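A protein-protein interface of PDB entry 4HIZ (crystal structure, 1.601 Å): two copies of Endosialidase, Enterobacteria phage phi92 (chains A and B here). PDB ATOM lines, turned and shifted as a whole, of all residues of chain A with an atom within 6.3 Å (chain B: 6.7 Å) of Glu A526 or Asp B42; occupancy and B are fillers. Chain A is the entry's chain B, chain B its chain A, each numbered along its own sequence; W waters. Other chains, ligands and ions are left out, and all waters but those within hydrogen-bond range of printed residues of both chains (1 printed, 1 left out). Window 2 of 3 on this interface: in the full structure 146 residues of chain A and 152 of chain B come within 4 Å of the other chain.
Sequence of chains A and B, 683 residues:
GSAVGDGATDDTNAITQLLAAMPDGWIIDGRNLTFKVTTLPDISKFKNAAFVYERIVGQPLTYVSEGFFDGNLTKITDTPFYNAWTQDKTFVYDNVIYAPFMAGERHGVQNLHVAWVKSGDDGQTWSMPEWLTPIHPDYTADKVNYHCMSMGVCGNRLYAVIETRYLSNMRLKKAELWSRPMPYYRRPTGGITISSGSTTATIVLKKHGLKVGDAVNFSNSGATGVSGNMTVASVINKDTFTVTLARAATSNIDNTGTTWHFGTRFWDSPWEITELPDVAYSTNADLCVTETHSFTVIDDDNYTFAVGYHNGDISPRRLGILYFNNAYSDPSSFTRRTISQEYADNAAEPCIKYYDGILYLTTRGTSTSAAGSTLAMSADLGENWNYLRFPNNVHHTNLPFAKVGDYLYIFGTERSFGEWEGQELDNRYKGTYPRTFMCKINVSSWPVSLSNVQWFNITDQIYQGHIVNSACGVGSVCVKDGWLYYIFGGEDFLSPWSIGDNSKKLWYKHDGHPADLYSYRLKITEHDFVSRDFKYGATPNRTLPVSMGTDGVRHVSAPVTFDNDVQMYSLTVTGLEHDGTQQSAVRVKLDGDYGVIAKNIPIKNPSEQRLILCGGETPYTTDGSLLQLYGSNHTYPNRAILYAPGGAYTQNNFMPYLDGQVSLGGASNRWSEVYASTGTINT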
ATOM      1  N   GLY A 482     -26.511  15.521  -4.542  1.00  0.00           N
ATOM      2  CA  GLY A 482     -25.090  15.548  -4.852  1.00  0.00           C
ATOM      3  C   GLY A 482     -24.602  14.464  -5.807  1.00  0.00           C
ATOM      4  O   GLY A 482     -23.391  14.214  -5.892  1.00  0.00           O
ATOM      5  N   LYS A 523     -20.180  11.756  -8.206  1.00  0.00           N
ATOM      6  CA  LYS A 523     -20.273  12.779  -7.180  1.00  0.00           C
ATOM      7  C   LYS A 523     -20.049  14.162  -7.785  1.00  0.00           C
ATOM      8  O   LYS A 523     -19.020  14.393  -8.431  1.00  0.00           O
ATOM      9  CB  LYS A 523     -19.212  12.481  -6.113  1.00  0.00           C
ATOM     10  CG  LYS A 523     -19.084  13.558  -5.042  1.00  0.00           C
ATOM     11  CD  LYS A 523     -18.075  13.065  -3.986  1.00  0.00           C
ATOM     12  CE  LYS A 523     -17.945  14.049  -2.820  1.00  0.00           C
ATOM     13  NZ  LYS A 523     -17.277  15.281  -3.315  1.00  0.00           N
ATOM     14  N   ILE A 524     -20.986  15.090  -7.558  1.00  0.00           N
ATOM     15  CA  ILE A 524     -20.870  16.422  -8.154  1.00  0.00           C
ATOM     16  C   ILE A 524     -20.939  17.580  -7.155  1.00  0.00           C
ATOM     17  O   ILE A 524     -20.854  18.738  -7.541  1.00  0.00           O
ATOM     18  CB  ILE A 524     -21.912  16.632  -9.305  1.00  0.00           C
ATOM     19  CG1 ILE A 524     -23.257  16.093  -8.820  1.00  0.00           C
ATOM     20  CG2 ILE A 524     -21.441  15.846 -10.582  1.00  0.00           C
ATOM     21  CD1 ILE A 524     -24.436  16.950  -8.956  1.00  0.00           C
ATOM     22  N   THR A 525     -21.095  17.285  -5.868  1.00  0.00           N
ATOM     23  CA  THR A 525     -21.022  18.308  -4.823  1.00  0.00           C
ATOM     24  C   THR A 525     -20.349  17.695  -3.597  1.00  0.00           C
ATOM     25  O   THR A 525     -20.077  16.484  -3.564  1.00  0.00           O
ATOM     26  CB  THR A 525     -22.420  18.794  -4.334  1.00  0.00           C
ATOM     27  OG1 THR A 525     -23.074  17.738  -3.618  1.00  0.00           O
ATOM     28  CG2 THR A 525     -23.312  19.280  -5.481  1.00  0.00           C
ATOM     29  N   GLU A 526     -20.127  18.506  -2.571  1.00  0.00           N
ATOM     30  CA  GLU A 526     -19.653  17.937  -1.293  1.00  0.00           C
ATOM     31  C   GLU A 526     -20.719  17.029  -0.733  1.00  0.00           C
ATOM     32  O   GLU A 526     -21.905  17.350  -0.838  1.00  0.00           O
ATOM     33  CB  GLU A 526     -19.317  19.035  -0.270  1.00  0.00           C
ATOM     34  CG  GLU A 526     -18.088  19.851  -0.679  1.00  0.00           C
ATOM     35  CD  GLU A 526     -17.602  20.843   0.381  1.00  0.00           C
ATOM     36  OE1 GLU A 526     -17.921  20.677   1.578  1.00  0.00           O
ATOM     37  OE2 GLU A 526     -16.883  21.797   0.009  1.00  0.00           O
ATOM     38  N   HIS A 527     -20.291  15.904  -0.144  1.00  0.00           N
ATOM     39  CA  HIS A 527     -21.200  15.016   0.574  1.00  0.00           C
ATOM     40  C   HIS A 527     -21.000  15.160   2.064  1.00  0.00           C
ATOM     41  O   HIS A 527     -20.186  14.460   2.662  1.00  0.00           O
ATOM     42  CB  HIS A 527     -20.996  13.575   0.110  1.00  0.00           C
ATOM     43  CG  HIS A 527     -21.468  13.346  -1.284  1.00  0.00           C
ATOM     44  ND1 HIS A 527     -21.352  12.128  -1.921  1.00  0.00           N
ATOM     45  CD2 HIS A 527     -22.064  14.182  -2.169  1.00  0.00           C
ATOM     46  CE1 HIS A 527     -21.857  12.224  -3.137  1.00  0.00           C
ATOM     47  NE2 HIS A 527     -22.290  13.459  -3.316  1.00  0.00           N
ATOM     48  N   ASP A 528     -21.757  16.093   2.650  1.00  0.00           N
ATOM     49  CA  ASP A 528     -21.586  16.470   4.046  1.00  0.00           C
ATOM     50  C   ASP A 528     -22.515  15.626   4.934  1.00  0.00           C
ATOM     51  O   ASP A 528     -23.348  16.135   5.703  1.00  0.00           O
ATOM     52  CB  ASP A 528     -21.834  17.973   4.223  1.00  0.00           C
ATOM     53  CG  ASP A 528     -23.215  18.398   3.761  1.00  0.00           C
ATOM     54  OD1 ASP A 528     -23.846  17.703   2.934  1.00  0.00           O
ATOM     55  OD2 ASP A 528     -23.676  19.458   4.219  1.00  0.00           O
ATOM     56  N   PHE A 529     -22.358  14.317   4.796  1.00  0.00           N
ATOM     57  CA  PHE A 529     -23.173  13.343   5.518  1.00  0.00           C
ATOM     58  C   PHE A 529     -22.415  12.039   5.564  1.00  0.00           C
ATOM     59  O   PHE A 529     -21.514  11.813   4.766  1.00  0.00           O
ATOM     60  CB  PHE A 529     -24.541  13.108   4.834  1.00  0.00           C
ATOM     61  CG  PHE A 529     -24.466  12.932   3.333  1.00  0.00           C
ATOM     62  CD1 PHE A 529     -24.159  11.703   2.783  1.00  0.00           C
ATOM     63  CD2 PHE A 529     -24.738  14.000   2.473  1.00  0.00           C
ATOM     64  CE1 PHE A 529     -24.074  11.512   1.377  1.00  0.00           C
ATOM     65  CE2 PHE A 529     -24.689  13.829   1.052  1.00  0.00           C
ATOM     66  CZ  PHE A 529     -24.338  12.572   0.507  1.00  0.00           C
ATOM     67  N   LEU B  40     -20.183  20.314   8.777  1.00  0.00           N
ATOM     68  CA  LEU B  40     -19.620  19.044   8.263  1.00  0.00           C
ATOM     69  C   LEU B  40     -18.866  19.279   6.974  1.00  0.00           C
ATOM     70  O   LEU B  40     -19.365  20.000   6.101  1.00  0.00           O
ATOM     71  CB  LEU B  40     -20.684  17.948   8.056  1.00  0.00           C
ATOM     72  CG  LEU B  40     -21.318  17.472   9.372  1.00  0.00           C
ATOM     73  CD1 LEU B  40     -22.406  16.447   9.105  1.00  0.00           C
ATOM     74  CD2 LEU B  40     -20.262  16.865  10.297  1.00  0.00           C
ATOM     75  N   PRO B  41     -17.671  18.666   6.839  1.00  0.00           N
ATOM     76  CA  PRO B  41     -16.889  18.813   5.615  1.00  0.00           C
ATOM     77  C   PRO B  41     -17.368  17.796   4.580  1.00  0.00           C
ATOM     78  O   PRO B  41     -18.409  17.161   4.765  1.00  0.00           O
ATOM     79  CB  PRO B  41     -15.479  18.473   6.086  1.00  0.00           C
ATOM     80  CG  PRO B  41     -15.703  17.365   7.099  1.00  0.00           C
ATOM     81  CD  PRO B  41     -16.976  17.812   7.841  1.00  0.00           C
ATOM     82  N   ASP B  42     -16.622  17.649   3.500  1.00  0.00           N
ATOM     83  CA  ASP B  42     -16.963  16.664   2.494  1.00  0.00           C
ATOM     84  C   ASP B  42     -16.495  15.296   3.012  1.00  0.00           C
ATOM     85  O   ASP B  42     -15.385  14.855   2.722  1.00  0.00           O
ATOM     86  CB  ASP B  42     -16.237  17.024   1.203  1.00  0.00           C
ATOM     87  CG  ASP B  42     -16.738  16.229   0.008  1.00  0.00           C
ATOM     88  OD1 ASP B  42     -17.519  15.268   0.192  1.00  0.00           O
ATOM     89  OD2 ASP B  42     -16.334  16.581  -1.119  1.00  0.00           O
ATOM     90  N   ILE B  43     -17.343  14.638   3.792  1.00  0.00           N
ATOM     91  CA  ILE B  43     -16.963  13.392   4.457  1.00  0.00           C
ATOM     92  C   ILE B  43     -16.470  12.292   3.500  1.00  0.00           C
ATOM     93  O   ILE B  43     -15.551  11.537   3.829  1.00  0.00           O
ATOM     94  CB  ILE B  43     -18.116  12.938   5.382  1.00  0.00           C
ATOM     95  CG1 ILE B  43     -18.272  13.945   6.515  1.00  0.00           C
ATOM     96  CG2 ILE B  43     -17.831  11.529   6.006  1.00  0.00           C
ATOM     97  CD1 ILE B  43     -19.542  13.707   7.340  1.00  0.00           C
ATOM     98  N   SER B  44     -17.020  12.245   2.288  1.00  0.00           N
ATOM     99  CA  SER B  44     -16.642  11.181   1.364  1.00  0.00           C
ATOM    100  C   SER B  44     -15.196  11.313   0.859  1.00  0.00           C
ATOM    101  O   SER B  44     -14.649  10.364   0.294  1.00  0.00           O
ATOM    102  CB  SER B  44     -17.615  11.133   0.192  1.00  0.00           C
ATOM    103  OG  SER B  44     -17.581  12.358  -0.491  1.00  0.00           O
ATOM    104  N   LYS B  45     -14.574  12.472   1.083  1.00  0.00           N
ATOM    105  CA  LYS B  45     -13.173  12.694   0.701  1.00  0.00           C
ATOM    106  C   LYS B  45     -12.166  12.357   1.820  1.00  0.00           C
ATOM    107  O   LYS B  45     -10.960  12.651   1.697  1.00  0.00           O
ATOM    108  CB  LYS B  45     -12.958  14.137   0.246  1.00  0.00           C
ATOM    109  CG  LYS B  45     -13.790  14.545  -0.972  1.00  0.00           C
ATOM    110  CD  LYS B  45     -13.642  13.555  -2.149  1.00  0.00           C
ATOM    111  CE  LYS B  45     -12.266  13.622  -2.804  1.00  0.00           C
ATOM    112  NZ  LYS B  45     -12.093  12.698  -3.999  1.00  0.00           N
ATOM    113  N   PHE B  46     -12.642  11.741   2.893  1.00  0.00           N
ATOM    114  CA  PHE B  46     -11.760  11.337   3.985  1.00  0.00           C
ATOM    115  C   PHE B  46     -11.837   9.834   4.128  1.00  0.00           C
ATOM    116  O   PHE B  46     -12.890   9.219   3.841  1.00  0.00           O
ATOM    117  CB  PHE B  46     -12.243  11.891   5.314  1.00  0.00           C
ATOM    118  CG  PHE B  46     -12.109  13.381   5.460  1.00  0.00           C
ATOM    119  CD1 PHE B  46     -13.044  14.232   4.883  1.00  0.00           C
ATOM    120  CD2 PHE B  46     -11.065  13.928   6.219  1.00  0.00           C
ATOM    121  CE1 PHE B  46     -12.950  15.620   5.051  1.00  0.00           C
ATOM    122  CE2 PHE B  46     -10.944  15.324   6.392  1.00  0.00           C
ATOM    123  CZ  PHE B  46     -11.886  16.172   5.808  1.00  0.00           C
ATOM    124  N   PHE B  51     -15.658  13.430  12.819  1.00  0.00           N
ATOM    125  CA  PHE B  51     -15.889  14.870  12.946  1.00  0.00           C
ATOM    126  C   PHE B  51     -16.923  15.122  14.030  1.00  0.00           C
ATOM    127  O   PHE B  51     -18.051  14.642  13.940  1.00  0.00           O
ATOM    128  CB  PHE B  51     -16.397  15.433  11.604  1.00  0.00           C
ATOM    129  CG  PHE B  51     -15.517  15.046  10.442  1.00  0.00           C
ATOM    130  CD1 PHE B  51     -14.368  15.762  10.165  1.00  0.00           C
ATOM    131  CD2 PHE B  51     -15.810  13.922   9.665  1.00  0.00           C
ATOM    132  CE1 PHE B  51     -13.526  15.381   9.103  1.00  0.00           C
ATOM    133  CE2 PHE B  51     -14.970  13.533   8.622  1.00  0.00           C
ATOM    134  CZ  PHE B  51     -13.824  14.267   8.349  1.00  0.00           C
HETATM  135  O   HOH W   1     -21.794  21.185   5.643  1.00  0.00           O
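The side-chain carboxylate (OD1) of Asp B42 lies within hydrogen-bond range of the side-chain hydroxyl (OG) of Ser B44 (3.0 Å). A ring nitrogen (NE2) of His A527 sits at hydrogen-bond distance from the backbone carbonyl oxygen (O) of Gly A482, at 2.9 Å. The side-chain amino group (NZ) of Lys A523 lies within hydrogen-bond range of the backbone carbonyl oxygen (O) of Thr A525 (3.1 Å).
No position is printed for both chains.
The side-chain carboxylate of Asp B42 lies within salt-bridge range of the side-chain amino group of Lys A523, 2.7 Å away. The side-chain carboxylate (OD1) of Asp B42 lies within hydrogen-bond range of the backbone NH (N) of His A527 (2.9 Å). N of Ile B43 is in hydrogen-bond range of O of His A527 (3.1 Å).
Of the 8 printed residues of chain A, 5 touch a printed residue of chain B. Hydrophobic or aromatic side chains of chain A within 4 Å of the printed part of chain B: His A527. Among the printed residues, Asp or Glu carboxylates within 4 Å of a Lys or Arg side-chain nitrogen of the other chain: Lys A523 with Asp B42.
Of chain B, only Asp B42 comes within 4 Å of Glu A526. Asp B42 touches just these residues of chain A: Lys A523 (2.7 Å), Glu A526 (3.6 Å) and His A527 (2.9 Å). Of the printed residues of chain A, Ile B43 touches His A527 (3.1 Å) and Phe A529 (3.6 Å). Printed residues of chain A within 4 Å of Pro B41: His A527 and Asp A528. Printed residues of chain B within 4 Å of His A527: Pro B41 (3.9 Å), Asp B42 (2.9 Å), Ile B43 (3.1 Å) and Ser B44 (3.7 Å). Phe B51 touches none of the printed residues of chain A.
Water W1 lies within hydrogen-bond range of O of Leu B40 (2.7 Å) and OD2 of Asp A528 (2.9 Å).
Lys A523 touches Ser B44. Glu A526 touches Asp B42. His A527 touches Pro B41 (O to O, 3.9 Å). Ser B44 touches His A527. Asp A528 touches Leu B40. Pro B41 touches Asp A528. Phe A529 touches Ile B43.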
